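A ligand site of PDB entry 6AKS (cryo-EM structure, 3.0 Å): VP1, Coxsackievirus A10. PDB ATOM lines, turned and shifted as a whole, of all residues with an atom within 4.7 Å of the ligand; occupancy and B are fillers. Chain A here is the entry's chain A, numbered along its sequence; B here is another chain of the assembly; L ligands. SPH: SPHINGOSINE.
An oxygen (O3) of the ligand is in hydrogen-bond range of the backbone NH of Ile 112 (2.9 Å).
N2 of the ligand lies within salt-bridge range of OD1 of Asp 111.
O of Tyr 152 is in hydrogen-bond range of N of Val 178 (2.7 Å).
N of Tyr 154 lies within hydrogen-bond range of O of Pro 176, at 3.1 Å.
The backbone NH of Met 194 sits at hydrogen-bond distance from the side-chain hydroxyl of Tyr 200, 3.3 Å away.
O of Val 189 sits at hydrogen-bond distance from N of Phe 134 (3.1 Å).
The side-chain carboxylate of Asp 111 is in hydrogen-bond range of the backbone NH of Met 113, at 3.1 Å.
Merely in contact with the ligand: Asn 227, Trp 202, Ile 110, Val 191, Met 194, Tyr 200, Met 229, Phe 134, Tyr 154, Met 113, Tyr 152 and Val 178.
Hydrophobic or aromatic side chains that line the ligand: Ile 110, Ile 112, Met 113, Phe 134, Tyr 154, Val 178, Val 191, Met 194, Trp 202 and Met 229.
Along chain A the residues within 4 Å of the ligand span positions 110 to 229.
The nearest printed residue that does not touch the ligand is Phe 136 (4.1 Å).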
ATOM      1  N   ILE A 110     -27.456  27.072  14.134  1.00  0.00           N
ATOM      2  CA  ILE A 110     -26.046  26.927  13.767  1.00  0.00           C
ATOM      3  C   ILE A 110     -25.823  25.476  13.370  1.00  0.00           C
ATOM      4  O   ILE A 110     -25.764  24.581  14.222  1.00  0.00           O
ATOM      5  CB  ILE A 110     -25.148  27.343  14.929  1.00  0.00           C
ATOM      6  CG1 ILE A 110     -25.348  28.822  15.199  1.00  0.00           C
ATOM      7  CG2 ILE A 110     -23.703  27.037  14.616  1.00  0.00           C
ATOM      8  CD1 ILE A 110     -24.766  29.254  16.483  1.00  0.00           C
ATOM      9  N   ASP A 111     -25.681  25.252  12.070  1.00  0.00           N
ATOM     10  CA  ASP A 111     -25.382  23.931  11.528  1.00  0.00           C
ATOM     11  C   ASP A 111     -24.424  24.182  10.378  1.00  0.00           C
ATOM     12  O   ASP A 111     -24.763  24.884   9.426  1.00  0.00           O
ATOM     13  CB  ASP A 111     -26.662  23.251  11.056  1.00  0.00           C
ATOM     14  CG  ASP A 111     -26.429  21.844  10.542  1.00  0.00           C
ATOM     15  OD1 ASP A 111     -25.272  21.366  10.582  1.00  0.00           O
ATOM     16  OD2 ASP A 111     -27.397  21.206  10.114  1.00  0.00           O
ATOM     17  N   ILE A 112     -23.229  23.596  10.445  1.00  0.00           N
ATOM     18  CA  ILE A 112     -22.221  23.934   9.458  1.00  0.00           C
ATOM     19  C   ILE A 112     -22.245  22.895   8.339  1.00  0.00           C
ATOM     20  O   ILE A 112     -21.443  22.958   7.404  1.00  0.00           O
ATOM     21  CB  ILE A 112     -20.839  24.083  10.105  1.00  0.00           C
ATOM     22  CG1 ILE A 112     -20.356  22.802  10.761  1.00  0.00           C
ATOM     23  CG2 ILE A 112     -20.908  25.178  11.148  1.00  0.00           C
ATOM     24  CD1 ILE A 112     -19.259  22.140   9.998  1.00  0.00           C
ATOM     25  N   MET A 113     -23.192  21.977   8.408  1.00  0.00           N
ATOM     26  CA  MET A 113     -23.394  20.956   7.394  1.00  0.00           C
ATOM     27  C   MET A 113     -24.179  21.479   6.205  1.00  0.00           C
ATOM     28  O   MET A 113     -24.447  20.719   5.272  1.00  0.00           O
ATOM     29  CB  MET A 113     -24.136  19.757   7.987  1.00  0.00           C
ATOM     30  CG  MET A 113     -23.402  18.998   9.085  1.00  0.00           C
ATOM     31  SD  MET A 113     -21.948  18.078   8.540  1.00  0.00           S
ATOM     32  CE  MET A 113     -20.616  19.058   9.208  1.00  0.00           C
ATOM     33  N   PHE A 130     -12.638  20.784  18.453  1.00  0.00           N
ATOM     34  CA  PHE A 130     -11.898  21.933  17.957  1.00  0.00           C
ATOM     35  C   PHE A 130     -12.415  23.206  18.606  1.00  0.00           C
ATOM     36  O   PHE A 130     -13.368  23.193  19.378  1.00  0.00           O
ATOM     37  CB  PHE A 130     -12.004  22.023  16.432  1.00  0.00           C
ATOM     38  CG  PHE A 130     -13.420  21.961  15.918  1.00  0.00           C
ATOM     39  CD1 PHE A 130     -14.199  23.088  15.837  1.00  0.00           C
ATOM     40  CD2 PHE A 130     -13.964  20.754  15.533  1.00  0.00           C
ATOM     41  CE1 PHE A 130     -15.485  23.024  15.386  1.00  0.00           C
ATOM     42  CE2 PHE A 130     -15.243  20.682  15.072  1.00  0.00           C
ATOM     43  CZ  PHE A 130     -16.006  21.821  14.994  1.00  0.00           C
ATOM     44  N   PHE A 134     -15.119  32.749  13.935  1.00  0.00           N
ATOM     45  CA  PHE A 134     -16.228  33.122  13.067  1.00  0.00           C
ATOM     46  C   PHE A 134     -16.063  34.556  12.595  1.00  0.00           C
ATOM     47  O   PHE A 134     -15.869  35.458  13.408  1.00  0.00           O
ATOM     48  CB  PHE A 134     -17.581  32.988  13.773  1.00  0.00           C
ATOM     49  CG  PHE A 134     -18.008  31.584  14.000  1.00  0.00           C
ATOM     50  CD1 PHE A 134     -18.699  30.899  13.022  1.00  0.00           C
ATOM     51  CD2 PHE A 134     -17.736  30.946  15.182  1.00  0.00           C
ATOM     52  CE1 PHE A 134     -19.092  29.607  13.230  1.00  0.00           C
ATOM     53  CE2 PHE A 134     -18.136  29.661  15.390  1.00  0.00           C
ATOM     54  CZ  PHE A 134     -18.810  28.989  14.404  1.00  0.00           C
ATOM     55  N   PHE A 136     -18.071  37.524  10.221  1.00  0.00           N
ATOM     56  CA  PHE A 136     -19.387  37.871   9.704  1.00  0.00           C
ATOM     57  C   PHE A 136     -19.213  38.949   8.645  1.00  0.00           C
ATOM     58  O   PHE A 136     -18.930  40.113   8.982  1.00  0.00           O
ATOM     59  CB  PHE A 136     -20.292  38.353  10.827  1.00  0.00           C
ATOM     60  CG  PHE A 136     -20.522  37.333  11.884  1.00  0.00           C
ATOM     61  CD1 PHE A 136     -21.506  36.388  11.746  1.00  0.00           C
ATOM     62  CD2 PHE A 136     -19.713  37.287  12.997  1.00  0.00           C
ATOM     63  CE1 PHE A 136     -21.681  35.432  12.703  1.00  0.00           C
ATOM     64  CE2 PHE A 136     -19.888  36.332  13.953  1.00  0.00           C
ATOM     65  CZ  PHE A 136     -20.883  35.403  13.805  1.00  0.00           C
ATOM     66  N   TYR A 152     -25.301  41.400  16.213  1.00  0.00           N
ATOM     67  CA  TYR A 152     -25.136  39.958  16.093  1.00  0.00           C
ATOM     68  C   TYR A 152     -25.172  39.355  17.489  1.00  0.00           C
ATOM     69  O   TYR A 152     -24.250  39.576  18.278  1.00  0.00           O
ATOM     70  CB  TYR A 152     -23.809  39.626  15.434  1.00  0.00           C
ATOM     71  CG  TYR A 152     -23.641  40.102  14.022  1.00  0.00           C
ATOM     72  CD1 TYR A 152     -24.625  39.910  13.088  1.00  0.00           C
ATOM     73  CD2 TYR A 152     -22.485  40.750  13.623  1.00  0.00           C
ATOM     74  CE1 TYR A 152     -24.470  40.328  11.802  1.00  0.00           C
ATOM     75  CE2 TYR A 152     -22.316  41.166  12.338  1.00  0.00           C
ATOM     76  CZ  TYR A 152     -23.319  40.960  11.432  1.00  0.00           C
ATOM     77  OH  TYR A 152     -23.155  41.384  10.147  1.00  0.00           O
ATOM     78  N   TYR A 154     -25.827  35.946  20.128  1.00  0.00           N
ATOM     79  CA  TYR A 154     -25.804  34.500  20.226  1.00  0.00           C
ATOM     80  C   TYR A 154     -26.843  34.078  21.255  1.00  0.00           C
ATOM     81  O   TYR A 154     -26.830  34.551  22.385  1.00  0.00           O
ATOM     82  CB  TYR A 154     -24.416  33.982  20.598  1.00  0.00           C
ATOM     83  CG  TYR A 154     -24.333  32.506  20.870  1.00  0.00           C
ATOM     84  CD1 TYR A 154     -24.661  31.579  19.900  1.00  0.00           C
ATOM     85  CD2 TYR A 154     -23.846  32.026  22.083  1.00  0.00           C
ATOM     86  CE1 TYR A 154     -24.593  30.229  20.149  1.00  0.00           C
ATOM     87  CE2 TYR A 154     -23.754  30.680  22.325  1.00  0.00           C
ATOM     88  CZ  TYR A 154     -24.133  29.790  21.353  1.00  0.00           C
ATOM     89  OH  TYR A 154     -24.043  28.443  21.604  1.00  0.00           O
ATOM     90  N   PRO A 176     -23.870  36.919  24.773  1.00  0.00           N
ATOM     91  CA  PRO A 176     -22.866  37.702  24.046  1.00  0.00           C
ATOM     92  C   PRO A 176     -23.427  38.327  22.775  1.00  0.00           C
ATOM     93  O   PRO A 176     -24.215  37.684  22.082  1.00  0.00           O
ATOM     94  CB  PRO A 176     -21.783  36.659  23.760  1.00  0.00           C
ATOM     95  CG  PRO A 176     -22.488  35.362  23.816  1.00  0.00           C
ATOM     96  CD  PRO A 176     -23.456  35.525  24.922  1.00  0.00           C
ATOM     97  N   VAL A 178     -22.497  41.263  19.345  1.00  0.00           N
ATOM     98  CA  VAL A 178     -21.540  42.111  18.629  1.00  0.00           C
ATOM     99  C   VAL A 178     -22.301  43.261  17.967  1.00  0.00           C
ATOM    100  O   VAL A 178     -23.296  43.036  17.272  1.00  0.00           O
ATOM    101  CB  VAL A 178     -20.734  41.321  17.587  1.00  0.00           C
ATOM    102  CG1 VAL A 178     -19.887  42.249  16.784  1.00  0.00           C
ATOM    103  CG2 VAL A 178     -19.842  40.329  18.272  1.00  0.00           C
ATOM    104  N   VAL A 189     -14.843  36.669  16.116  1.00  0.00           N
ATOM    105  CA  VAL A 189     -14.796  36.226  17.511  1.00  0.00           C
ATOM    106  C   VAL A 189     -14.208  34.822  17.555  1.00  0.00           C
ATOM    107  O   VAL A 189     -14.176  34.109  16.554  1.00  0.00           O
ATOM    108  CB  VAL A 189     -16.178  36.207  18.181  1.00  0.00           C
ATOM    109  CG1 VAL A 189     -16.793  37.580  18.223  1.00  0.00           C
ATOM    110  CG2 VAL A 189     -17.078  35.246  17.456  1.00  0.00           C
ATOM    111  N   VAL A 191     -14.600  31.107  19.504  1.00  0.00           N
ATOM    112  CA  VAL A 191     -15.621  30.312  20.148  1.00  0.00           C
ATOM    113  C   VAL A 191     -14.946  29.061  20.704  1.00  0.00           C
ATOM    114  O   VAL A 191     -14.016  28.562  20.086  1.00  0.00           O
ATOM    115  CB  VAL A 191     -16.759  29.944  19.177  1.00  0.00           C
ATOM    116  CG1 VAL A 191     -17.822  29.130  19.856  1.00  0.00           C
ATOM    117  CG2 VAL A 191     -17.353  31.193  18.589  1.00  0.00           C
ATOM    118  N   MET A 194     -17.995  23.708  22.821  1.00  0.00           N
ATOM    119  CA  MET A 194     -19.150  23.795  23.702  1.00  0.00           C
ATOM    120  C   MET A 194     -19.950  22.514  23.821  1.00  0.00           C
ATOM    121  O   MET A 194     -20.985  22.514  24.496  1.00  0.00           O
ATOM    122  CB  MET A 194     -20.053  24.941  23.267  1.00  0.00           C
ATOM    123  CG  MET A 194     -19.414  26.292  23.480  1.00  0.00           C
ATOM    124  SD  MET A 194     -20.556  27.636  23.257  1.00  0.00           S
ATOM    125  CE  MET A 194     -20.802  27.522  21.494  1.00  0.00           C
ATOM    126  N   TYR A 200     -17.408  16.582  19.211  1.00  0.00           N
ATOM    127  CA  TYR A 200     -18.456  16.627  18.206  1.00  0.00           C
ATOM    128  C   TYR A 200     -18.435  15.324  17.427  1.00  0.00           C
ATOM    129  O   TYR A 200     -17.392  14.700  17.275  1.00  0.00           O
ATOM    130  CB  TYR A 200     -18.235  17.790  17.258  1.00  0.00           C
ATOM    131  CG  TYR A 200     -18.269  19.157  17.890  1.00  0.00           C
ATOM    132  CD1 TYR A 200     -19.305  19.554  18.712  1.00  0.00           C
ATOM    133  CD2 TYR A 200     -17.224  20.034  17.697  1.00  0.00           C
ATOM    134  CE1 TYR A 200     -19.316  20.801  19.277  1.00  0.00           C
ATOM    135  CE2 TYR A 200     -17.228  21.274  18.252  1.00  0.00           C
ATOM    136  CZ  TYR A 200     -18.272  21.652  19.052  1.00  0.00           C
ATOM    137  OH  TYR A 200     -18.246  22.902  19.601  1.00  0.00           O
ATOM    138  N   TRP A 202     -20.124  13.746  13.735  1.00  0.00           N
ATOM    139  CA  TRP A 202     -20.890  14.072  12.554  1.00  0.00           C
ATOM    140  C   TRP A 202     -21.782  12.920  12.140  1.00  0.00           C
ATOM    141  O   TRP A 202     -22.591  13.079  11.226  1.00  0.00           O
ATOM    142  CB  TRP A 202     -19.971  14.444  11.400  1.00  0.00           C
ATOM    143  CG  TRP A 202     -18.927  15.410  11.797  1.00  0.00           C
ATOM    144  CD1 TRP A 202     -17.592  15.211  11.782  1.00  0.00           C
ATOM    145  CD2 TRP A 202     -19.134  16.675  12.415  1.00  0.00           C
ATOM    146  NE1 TRP A 202     -16.943  16.309  12.260  1.00  0.00           N
ATOM    147  CE2 TRP A 202     -17.872  17.217  12.684  1.00  0.00           C
ATOM    148  CE3 TRP A 202     -20.270  17.406  12.756  1.00  0.00           C
ATOM    149  CZ2 TRP A 202     -17.720  18.460  13.265  1.00  0.00           C
ATOM    150  CZ3 TRP A 202     -20.106  18.632  13.337  1.00  0.00           C
ATOM    151  CH2 TRP A 202     -18.845  19.149  13.574  1.00  0.00           C
ATOM    152  N   ASN A 227     -24.881  18.132  19.305  1.00  0.00           N
ATOM    153  CA  ASN A 227     -24.483  19.127  18.333  1.00  0.00           C
ATOM    154  C   ASN A 227     -25.334  20.375  18.313  1.00  0.00           C
ATOM    155  O   ASN A 227     -25.104  21.234  17.466  1.00  0.00           O
ATOM    156  CB  ASN A 227     -24.486  18.510  16.922  1.00  0.00           C
ATOM    157  CG  ASN A 227     -23.431  17.448  16.752  1.00  0.00           C
ATOM    158  OD1 ASN A 227     -23.695  16.384  16.203  1.00  0.00           O
ATOM    159  ND2 ASN A 227     -22.233  17.709  17.238  1.00  0.00           N
ATOM    160  N   MET A 229     -26.189  23.795  19.203  1.00  0.00           N
ATOM    161  CA  MET A 229     -25.398  24.886  19.766  1.00  0.00           C
ATOM    162  C   MET A 229     -26.180  26.161  19.996  1.00  0.00           C
ATOM    163  O   MET A 229     -25.585  27.158  20.402  1.00  0.00           O
ATOM    164  CB  MET A 229     -24.205  25.162  18.852  1.00  0.00           C
ATOM    165  CG  MET A 229     -23.185  24.037  18.806  1.00  0.00           C
ATOM    166  SD  MET A 229     -22.336  23.811  20.373  1.00  0.00           S
ATOM    167  CE  MET A 229     -23.098  22.313  20.975  1.00  0.00           C
ATOM    168  N   PHE A 232     -28.187  31.915  16.097  1.00  0.00           N
ATOM    169  CA  PHE A 232     -27.577  33.205  15.779  1.00  0.00           C
ATOM    170  C   PHE A 232     -28.648  34.115  15.202  1.00  0.00           C
ATOM    171  O   PHE A 232     -29.406  33.704  14.326  1.00  0.00           O
ATOM    172  CB  PHE A 232     -26.422  33.018  14.801  1.00  0.00           C
ATOM    173  CG  PHE A 232     -25.899  34.292  14.212  1.00  0.00           C
ATOM    174  CD1 PHE A 232     -25.023  35.087  14.913  1.00  0.00           C
ATOM    175  CD2 PHE A 232     -26.268  34.673  12.943  1.00  0.00           C
ATOM    176  CE1 PHE A 232     -24.542  36.243  14.362  1.00  0.00           C
ATOM    177  CE2 PHE A 232     -25.782  35.821  12.402  1.00  0.00           C
ATOM    178  CZ  PHE A 232     -24.923  36.603  13.101  1.00  0.00           C
ATOM    179  N   MET A 252     -16.442  29.933   9.088  1.00  0.00           N
ATOM    180  CA  MET A 252     -15.913  29.284  10.274  1.00  0.00           C
ATOM    181  C   MET A 252     -14.527  28.712   9.988  1.00  0.00           C
ATOM    182  O   MET A 252     -14.324  28.002   9.004  1.00  0.00           O
ATOM    183  CB  MET A 252     -16.834  28.177  10.766  1.00  0.00           C
ATOM    184  CG  MET A 252     -16.335  27.458  11.995  1.00  0.00           C
ATOM    185  SD  MET A 252     -17.447  26.198  12.608  1.00  0.00           S
ATOM    186  CE  MET A 252     -17.198  24.949  11.361  1.00  0.00           C
ATOM    187  N   ILE B  24     -15.769  34.731  23.147  1.00  0.00           N
ATOM    188  CA  ILE B  24     -17.147  35.061  23.488  1.00  0.00           C
ATOM    189  C   ILE B  24     -17.425  34.789  24.963  1.00  0.00           C
ATOM    190  O   ILE B  24     -18.214  35.503  25.579  1.00  0.00           O
ATOM    191  CB  ILE B  24     -18.130  34.299  22.587  1.00  0.00           C
ATOM    192  CG1 ILE B  24     -17.981  32.797  22.783  1.00  0.00           C
ATOM    193  CG2 ILE B  24     -17.883  34.635  21.163  1.00  0.00           C
ATOM    194  CD1 ILE B  24     -19.061  32.001  22.122  1.00  0.00           C
HETATM  195  C1  SPH L   1     -24.996  20.978  14.328  1.00  0.00           C
HETATM  196  O1  SPH L   1     -26.122  20.150  14.144  1.00  0.00           O
HETATM  197  C2  SPH L   1     -23.751  20.190  13.954  1.00  0.00           C
HETATM  198  N2  SPH L   1     -24.154  19.282  12.897  1.00  0.00           N
HETATM  199  C3  SPH L   1     -22.633  21.095  13.468  1.00  0.00           C
HETATM  200  O3  SPH L   1     -23.196  22.330  13.083  1.00  0.00           O
HETATM  201  C4  SPH L   1     -21.561  21.352  14.505  1.00  0.00           C
HETATM  202  C5  SPH L   1     -21.632  22.446  15.477  1.00  0.00           C
HETATM  203  C6  SPH L   1     -21.059  23.807  15.150  1.00  0.00           C
HETATM  204  C7  SPH L   1     -19.600  23.987  15.545  1.00  0.00           C
HETATM  205  C8  SPH L   1     -19.412  24.862  16.790  1.00  0.00           C
HETATM  206  C9  SPH L   1     -20.089  26.213  16.683  1.00  0.00           C
HETATM  207  C10 SPH L   1     -20.593  26.717  18.027  1.00  0.00           C
HETATM  208  C11 SPH L   1     -21.550  27.912  17.893  1.00  0.00           C
HETATM  209  C12 SPH L   1     -20.864  29.259  18.140  1.00  0.00           C
HETATM  210  C13 SPH L   1     -21.702  30.429  17.653  1.00  0.00           C
HETATM  211  C14 SPH L   1     -21.200  31.767  18.184  1.00  0.00           C
HETATM  212  C15 SPH L   1     -21.703  32.969  17.379  1.00  0.00           C
HETATM  213  C16 SPH L   1     -21.169  34.257  18.021  1.00  0.00           C
HETATM  214  C17 SPH L   1     -21.995  35.497  17.701  1.00  0.00           C
HETATM  215  C18 SPH L   1     -21.495  36.699  18.494  1.00  0.00           C
